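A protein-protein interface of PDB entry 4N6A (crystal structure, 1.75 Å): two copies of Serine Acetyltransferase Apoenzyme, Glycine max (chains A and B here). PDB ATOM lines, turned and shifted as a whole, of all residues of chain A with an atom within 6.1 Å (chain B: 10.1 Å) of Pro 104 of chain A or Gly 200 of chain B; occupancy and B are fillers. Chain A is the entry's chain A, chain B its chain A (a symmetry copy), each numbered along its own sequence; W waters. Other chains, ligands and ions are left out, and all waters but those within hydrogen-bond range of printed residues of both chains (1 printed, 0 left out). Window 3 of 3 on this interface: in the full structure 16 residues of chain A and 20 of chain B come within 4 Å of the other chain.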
ATOM      1  N   ALA A  99      -6.981  -2.962   5.786  1.00  0.00           N
ATOM      2  CA  ALA A  99      -6.081  -4.035   6.226  1.00  0.00           C
ATOM      3  C   ALA A  99      -6.482  -5.380   5.615  1.00  0.00           C
ATOM      4  O   ALA A  99      -5.638  -6.120   5.099  1.00  0.00           O
ATOM      5  CB  ALA A  99      -6.059  -4.131   7.759  1.00  0.00           C
ATOM      6  N   ARG A 102      -5.599  -5.050   1.724  1.00  0.00           N
ATOM      7  CA  ARG A 102      -4.274  -4.664   1.236  1.00  0.00           C
ATOM      8  C   ARG A 102      -3.086  -5.187   2.048  1.00  0.00           C
ATOM      9  O   ARG A 102      -1.959  -5.166   1.559  1.00  0.00           O
ATOM     10  CB  ARG A 102      -4.176  -3.138   1.183  1.00  0.00           C
ATOM     11  CG  ARG A 102      -4.756  -2.498  -0.048  1.00  0.00           C
ATOM     12  CD  ARG A 102      -4.516  -1.002  -0.013  1.00  0.00           C
ATOM     13  NE  ARG A 102      -5.703  -0.305   0.444  1.00  0.00           N
ATOM     14  CZ  ARG A 102      -5.699   0.745   1.253  1.00  0.00           C
ATOM     15  NH1 ARG A 102      -4.558   1.252   1.708  1.00  0.00           N
ATOM     16  NH2 ARG A 102      -6.848   1.297   1.593  1.00  0.00           N
ATOM     17  N   ASP A 103      -3.316  -5.607   3.293  1.00  0.00           N
ATOM     18  CA  ASP A 103      -2.218  -6.081   4.138  1.00  0.00           C
ATOM     19  C   ASP A 103      -1.556  -7.295   3.522  1.00  0.00           C
ATOM     20  O   ASP A 103      -2.216  -8.300   3.287  1.00  0.00           O
ATOM     21  CB  ASP A 103      -2.699  -6.435   5.547  1.00  0.00           C
ATOM     22  CG  ASP A 103      -1.593  -7.023   6.413  1.00  0.00           C
ATOM     23  OD1 ASP A 103      -0.508  -6.415   6.496  1.00  0.00           O
ATOM     24  OD2 ASP A 103      -1.803  -8.102   7.009  1.00  0.00           O
ATOM     25  N   PRO A 104      -0.244  -7.204   3.264  1.00  0.00           N
ATOM     26  CA  PRO A 104       0.521  -8.306   2.674  1.00  0.00           C
ATOM     27  C   PRO A 104       0.466  -9.573   3.526  1.00  0.00           C
ATOM     28  O   PRO A 104       0.535 -10.674   2.984  1.00  0.00           O
ATOM     29  CB  PRO A 104       1.949  -7.752   2.613  1.00  0.00           C
ATOM     30  CG  PRO A 104       1.782  -6.263   2.625  1.00  0.00           C
ATOM     31  CD  PRO A 104       0.595  -6.015   3.497  1.00  0.00           C
ATOM     32  N   ALA A 105       0.333  -9.413   4.840  1.00  0.00           N
ATOM     33  CA  ALA A 105       0.267 -10.558   5.738  1.00  0.00           C
ATOM     34  C   ALA A 105      -1.154 -11.114   5.846  1.00  0.00           C
ATOM     35  O   ALA A 105      -1.405 -12.039   6.616  1.00  0.00           O
ATOM     36  CB  ALA A 105       0.795 -10.182   7.118  1.00  0.00           C
ATOM     37  N   CYS A 106      -2.070 -10.534   5.072  1.00  0.00           N
ATOM     38  CA  CYS A 106      -3.457 -11.000   4.977  1.00  0.00           C
ATOM     39  C   CYS A 106      -4.147 -11.199   6.333  1.00  0.00           C
ATOM     40  O   CYS A 106      -4.299 -12.329   6.800  1.00  0.00           O
ATOM     41  CB  CYS A 106      -3.509 -12.314   4.196  1.00  0.00           C
ATOM     42  SG  CYS A 106      -2.624 -12.290   2.623  1.00  0.00           S
ATOM     43  N   LEU A 166      -3.409   2.133   5.585  1.00  0.00           N
ATOM     44  CA  LEU A 166      -2.670   0.915   5.903  1.00  0.00           C
ATOM     45  C   LEU A 166      -1.295   1.284   6.449  1.00  0.00           C
ATOM     46  O   LEU A 166      -0.507   1.941   5.766  1.00  0.00           O
ATOM     47  CB  LEU A 166      -2.540   0.019   4.669  1.00  0.00           C
ATOM     48  CG  LEU A 166      -1.869  -1.329   4.971  1.00  0.00           C
ATOM     49  CD1 LEU A 166      -2.822  -2.258   5.724  1.00  0.00           C
ATOM     50  CD2 LEU A 166      -1.346  -2.005   3.726  1.00  0.00           C
ATOM     51  N   ASP A 168       1.763  -0.582   7.705  1.00  0.00           N
ATOM     52  CA  ASP A 168       2.500  -1.843   7.782  1.00  0.00           C
ATOM     53  C   ASP A 168       3.814  -1.753   8.566  1.00  0.00           C
ATOM     54  O   ASP A 168       4.721  -0.998   8.202  1.00  0.00           O
ATOM     55  CB  ASP A 168       2.783  -2.357   6.371  1.00  0.00           C
ATOM     56  CG  ASP A 168       3.626  -3.612   6.367  1.00  0.00           C
ATOM     57  OD1 ASP A 168       3.151  -4.648   6.879  1.00  0.00           O
ATOM     58  OD2 ASP A 168       4.759  -3.564   5.841  1.00  0.00           O
ATOM     59  N   HIS B 156       8.254 -12.177  12.819  1.00  0.00           N
ATOM     60  CA  HIS B 156       7.004 -12.937  12.709  1.00  0.00           C
ATOM     61  C   HIS B 156       7.219 -14.376  13.193  1.00  0.00           C
ATOM     62  O   HIS B 156       8.252 -14.966  12.918  1.00  0.00           O
ATOM     63  CB  HIS B 156       6.485 -12.931  11.266  1.00  0.00           C
ATOM     64  CG  HIS B 156       5.092 -13.457  11.133  1.00  0.00           C
ATOM     65  ND1 HIS B 156       4.805 -14.805  11.112  1.00  0.00           N
ATOM     66  CD2 HIS B 156       3.899 -12.819  11.065  1.00  0.00           C
ATOM     67  CE1 HIS B 156       3.498 -14.974  11.012  1.00  0.00           C
ATOM     68  NE2 HIS B 156       2.925 -13.783  10.985  1.00  0.00           N
ATOM     69  N   GLY B 176      10.289 -10.407   8.387  1.00  0.00           N
ATOM     70  CA  GLY B 176       8.975 -10.750   7.891  1.00  0.00           C
ATOM     71  C   GLY B 176       8.627 -12.222   7.925  1.00  0.00           C
ATOM     72  O   GLY B 176       9.495 -13.085   8.097  1.00  0.00           O
ATOM     73  N   GLU B 177       7.339 -12.483   7.715  1.00  0.00           N
ATOM     74  CA  GLU B 177       6.717 -13.796   7.827  1.00  0.00           C
ATOM     75  C   GLU B 177       7.391 -14.924   7.059  1.00  0.00           C
ATOM     76  O   GLU B 177       7.399 -16.062   7.521  1.00  0.00           O
ATOM     77  CB  GLU B 177       5.262 -13.680   7.371  1.00  0.00           C
ATOM     78  CG  GLU B 177       4.458 -14.955   7.408  1.00  0.00           C
ATOM     79  CD  GLU B 177       2.983 -14.689   7.183  1.00  0.00           C
ATOM     80  OE1 GLU B 177       2.162 -15.534   7.592  1.00  0.00           O
ATOM     81  OE2 GLU B 177       2.648 -13.628   6.611  1.00  0.00           O
ATOM     82  N   THR B 178       7.937 -14.629   5.884  1.00  0.00           N
ATOM     83  CA  THR B 178       8.499 -15.688   5.057  1.00  0.00           C
ATOM     84  C   THR B 178      10.020 -15.604   5.000  1.00  0.00           C
ATOM     85  O   THR B 178      10.656 -16.237   4.157  1.00  0.00           O
ATOM     86  CB  THR B 178       7.913 -15.653   3.621  1.00  0.00           C
ATOM     87  OG1 THR B 178       8.279 -14.424   2.972  1.00  0.00           O
ATOM     88  CG2 THR B 178       6.388 -15.786   3.662  1.00  0.00           C
ATOM     89  N   GLY B 194      12.106  -7.616   4.885  1.00  0.00           N
ATOM     90  CA  GLY B 194      10.681  -7.499   4.626  1.00  0.00           C
ATOM     91  C   GLY B 194      10.316  -7.470   3.152  1.00  0.00           C
ATOM     92  O   GLY B 194      11.023  -8.022   2.313  1.00  0.00           O
ATOM     93  N   GLY B 195       9.205  -6.813   2.835  1.00  0.00           N
ATOM     94  CA  GLY B 195       8.645  -6.891   1.498  1.00  0.00           C
ATOM     95  C   GLY B 195       8.317  -5.573   0.821  1.00  0.00           C
ATOM     96  O   GLY B 195       8.475  -4.500   1.404  1.00  0.00           O
ATOM     97  N   THR B 196       7.837  -5.665  -0.417  1.00  0.00           N
ATOM     98  CA  THR B 196       7.608  -4.507  -1.273  1.00  0.00           C
ATOM     99  C   THR B 196       6.289  -3.801  -0.966  1.00  0.00           C
ATOM    100  O   THR B 196       6.116  -2.627  -1.290  1.00  0.00           O
ATOM    101  CB  THR B 196       7.607  -4.926  -2.764  1.00  0.00           C
ATOM    102  OG1 THR B 196       6.722  -6.040  -2.949  1.00  0.00           O
ATOM    103  CG2 THR B 196       9.005  -5.350  -3.192  1.00  0.00           C
ATOM    104  N   GLY B 197       5.359  -4.527  -0.357  1.00  0.00           N
ATOM    105  CA  GLY B 197       3.992  -4.062  -0.223  1.00  0.00           C
ATOM    106  C   GLY B 197       3.098  -5.010  -1.000  1.00  0.00           C
ATOM    107  O   GLY B 197       1.873  -4.932  -0.916  1.00  0.00           O
ATOM    108  N   LYS B 198       3.729  -5.901  -1.766  1.00  0.00           N
ATOM    109  CA  LYS B 198       3.034  -6.971  -2.479  1.00  0.00           C
ATOM    110  C   LYS B 198       2.297  -7.883  -1.500  1.00  0.00           C
ATOM    111  O   LYS B 198       2.846  -8.271  -0.471  1.00  0.00           O
ATOM    112  CB  LYS B 198       4.025  -7.791  -3.314  1.00  0.00           C
ATOM    113  CG  LYS B 198       3.653  -9.261  -3.433  1.00  0.00           C
ATOM    114  CD  LYS B 198       4.713 -10.070  -4.157  1.00  0.00           C
ATOM    115  CE  LYS B 198       4.166 -11.429  -4.564  1.00  0.00           C
ATOM    116  NZ  LYS B 198       3.041 -11.858  -3.683  1.00  0.00           N
ATOM    117  N   VAL B 199       1.055  -8.221  -1.829  1.00  0.00           N
ATOM    118  CA  VAL B 199       0.221  -9.021  -0.939  1.00  0.00           C
ATOM    119  C   VAL B 199       0.393 -10.531  -1.136  1.00  0.00           C
ATOM    120  O   VAL B 199       0.353 -11.038  -2.259  1.00  0.00           O
ATOM    121  CB  VAL B 199      -1.270  -8.659  -1.111  1.00  0.00           C
ATOM    122  CG1 VAL B 199      -2.109  -9.346  -0.049  1.00  0.00           C
ATOM    123  CG2 VAL B 199      -1.454  -7.152  -1.023  1.00  0.00           C
ATOM    124  N   GLY B 200       0.593 -11.235  -0.024  1.00  0.00           N
ATOM    125  CA  GLY B 200       0.602 -12.686  -0.011  1.00  0.00           C
ATOM    126  C   GLY B 200       1.891 -13.342  -0.467  1.00  0.00           C
ATOM    127  O   GLY B 200       2.751 -12.704  -1.075  1.00  0.00           O
ATOM    128  N   GLY B 201       2.021 -14.626  -0.149  1.00  0.00           N
ATOM    129  CA  GLY B 201       3.085 -15.460  -0.680  1.00  0.00           C
ATOM    130  C   GLY B 201       4.481 -15.195  -0.155  1.00  0.00           C
ATOM    131  O   GLY B 201       4.688 -14.364   0.734  1.00  0.00           O
ATOM    132  N   ASP B 202       5.445 -15.918  -0.721  1.00  0.00           N
ATOM    133  CA  ASP B 202       6.848 -15.799  -0.349  1.00  0.00           C
ATOM    134  C   ASP B 202       7.410 -14.469  -0.842  1.00  0.00           C
ATOM    135  O   ASP B 202       7.580 -14.267  -2.045  1.00  0.00           O
ATOM    136  CB  ASP B 202       7.644 -16.973  -0.925  1.00  0.00           C
ATOM    137  CG  ASP B 202       8.923 -17.246  -0.161  1.00  0.00           C
ATOM    138  OD1 ASP B 202       9.421 -16.329   0.526  1.00  0.00           O
ATOM    139  OD2 ASP B 202       9.439 -18.380  -0.255  1.00  0.00           O
ATOM    140  N   ARG B 203       7.710 -13.571   0.093  1.00  0.00           N
ATOM    141  CA  ARG B 203       8.009 -12.184  -0.246  1.00  0.00           C
ATOM    142  C   ARG B 203       9.115 -11.581   0.619  1.00  0.00           C
ATOM    143  O   ARG B 203       9.353 -10.372   0.571  1.00  0.00           O
ATOM    144  CB  ARG B 203       6.738 -11.340  -0.112  1.00  0.00           C
ATOM    145  CG  ARG B 203       6.141 -11.384   1.291  1.00  0.00           C
ATOM    146  CD  ARG B 203       4.715 -10.851   1.332  1.00  0.00           C
ATOM    147  NE  ARG B 203       4.262 -10.652   2.706  1.00  0.00           N
ATOM    148  CZ  ARG B 203       3.785 -11.618   3.487  1.00  0.00           C
ATOM    149  NH1 ARG B 203       3.691 -12.861   3.030  1.00  0.00           N
ATOM    150  NH2 ARG B 203       3.403 -11.339   4.728  1.00  0.00           N
ATOM    151  N   HIS B 204       9.782 -12.418   1.409  1.00  0.00           N
ATOM    152  CA  HIS B 204      10.812 -11.952   2.333  1.00  0.00           C
ATOM    153  C   HIS B 204      12.149 -12.679   2.101  1.00  0.00           C
ATOM    154  O   HIS B 204      12.174 -13.804   1.608  1.00  0.00           O
ATOM    155  CB  HIS B 204      10.322 -12.123   3.777  1.00  0.00           C
ATOM    156  CG  HIS B 204       9.044 -11.391   4.063  1.00  0.00           C
ATOM    157  ND1 HIS B 204       7.965 -11.993   4.677  1.00  0.00           N
ATOM    158  CD2 HIS B 204       8.670 -10.119   3.805  1.00  0.00           C
ATOM    159  CE1 HIS B 204       6.984 -11.114   4.792  1.00  0.00           C
ATOM    160  NE2 HIS B 204       7.384  -9.969   4.273  1.00  0.00           N
ATOM    161  N   GLY B 221      11.921  -8.346  -0.670  1.00  0.00           N
ATOM    162  CA  GLY B 221      11.547  -9.311  -1.684  1.00  0.00           C
ATOM    163  C   GLY B 221      12.114 -10.664  -1.318  1.00  0.00           C
ATOM    164  O   GLY B 221      12.917 -10.763  -0.406  1.00  0.00           O
ATOM    165  N   ASN B 222      11.692 -11.713  -2.007  1.00  0.00           N
ATOM    166  CA  ASN B 222      12.293 -13.007  -1.783  1.00  0.00           C
ATOM    167  C   ASN B 222      13.549 -13.112  -2.632  1.00  0.00           C
ATOM    168  O   ASN B 222      13.536 -13.693  -3.715  1.00  0.00           O
ATOM    169  CB  ASN B 222      11.316 -14.130  -2.113  1.00  0.00           C
ATOM    170  CG  ASN B 222      11.838 -15.484  -1.707  1.00  0.00           C
ATOM    171  OD1 ASN B 222      12.784 -15.581  -0.927  1.00  0.00           O
ATOM    172  ND2 ASN B 222      11.232 -16.541  -2.239  1.00  0.00           N
HETATM  173  O   HOH W   1      -0.745  -3.580  -0.343  1.00  0.00           O
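The backbone NH of Ala 105 of chain A sits close to the side-chain carboxylate of Asp 103 of chain A, 3.3 Å away.
The side-chain carboxylate of Asp 103 of chain A lies within hydrogen-bond range of the backbone NH of Cys 106 of chain A (3.1 Å).
The side-chain sulfur (SG) of Cys 106 of chain A lies within hydrogen-bond range of the backbone carbonyl oxygen (O) of Pro 104 of chain A.
The backbone NH of Glu 177 of chain B lies within hydrogen-bond range of a ring nitrogen (ND1) of His 204 of chain B.
The backbone NH (N) of Arg 203 of chain B is in hydrogen-bond range of the side-chain hydroxyl (OG1) of Thr 178 of chain B (3.1 Å).
The backbone carbonyl oxygen of Arg 203 of chain B sits close to the backbone NH of Gly 221 of chain B (3.5 Å).
Pro 104 of chain A touches just these residues of chain B: Gly 197 (3.8 Å), Lys 198 (3.3 Å), Val 199 (3.7 Å), Gly 200 (3.1 Å) and Arg 203 (3.4 Å).
Of chain B, only Glu 177 and Arg 203 come within 4 Å of Ala 105 of chain A.
Printed residues of chain A within 4 Å of Gly 197 of chain B: Pro 104.
Of the printed residues of chain A, Lys 198 of chain B touches Pro 104.
Printed residues of chain A within 4 Å of Val 199 of chain B: Arg 102, Asp 103 and Pro 104.
Printed residues of chain A within 4 Å of Gly 200 of chain B: Pro 104.
Printed residues of chain A within 4 Å of Arg 203 of chain B: Pro 104 (3.4 Å) and Ala 105 (3.4 Å).
The nearest printed residue of chain A that does not touch Val 199 of chain B is Cys 106 of chain A (4.01 Å).
Printed residues of chain B that touch a printed residue of chain A: Glu 177, Gly 197, Lys 198, Val 199, Gly 200 and Arg 203.
Printed residues of chain A that touch a printed residue of chain B: Arg 102, Asp 103, Pro 104 and Ala 105.
Hydrophobic or aromatic side chains of chain A within 4 Å of the printed part of chain B: Pro 104 and Ala 105.
Among the printed residues, no Asp or Glu carboxylate lies within 4 Å of a Lys or Arg side-chain nitrogen of the other chain.
Water W1 lies within hydrogen-bond range of the backbone carbonyl oxygen (O) of Arg 102 of chain A (2.8 Å) and the backbone carbonyl oxygen (O) of Gly 197 of chain B (3.0 Å).
O of Pro 104 of chain A lies within hydrogen-bond range of N of Gly 200 of chain B (3.1 Å).
The backbone carbonyl oxygen (O) of Pro 104 of chain A sits close to the guanidinium group (NH2) of Arg 203 of chain B.
Among the printed residues, merely in contact across the chains: Arg 102 of chain A with Val 199 of chain B (3.3 Å), Asp 103 of chain A with Val 199 of chain B (3.5 Å), Pro 104 of chain A with Gly 197 of chain B (3.8 Å), Pro 104 of chain A with Lys 198 of chain B (3.3 Å), Pro 104 of chain A with Val 199 of chain B (3.7 Å), Ala 105 of chain A with Glu 177 of chain B (3.9 Å) and Ala 105 of chain A with Arg 203 of chain B (3.4 Å).
No position is printed for both chains.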
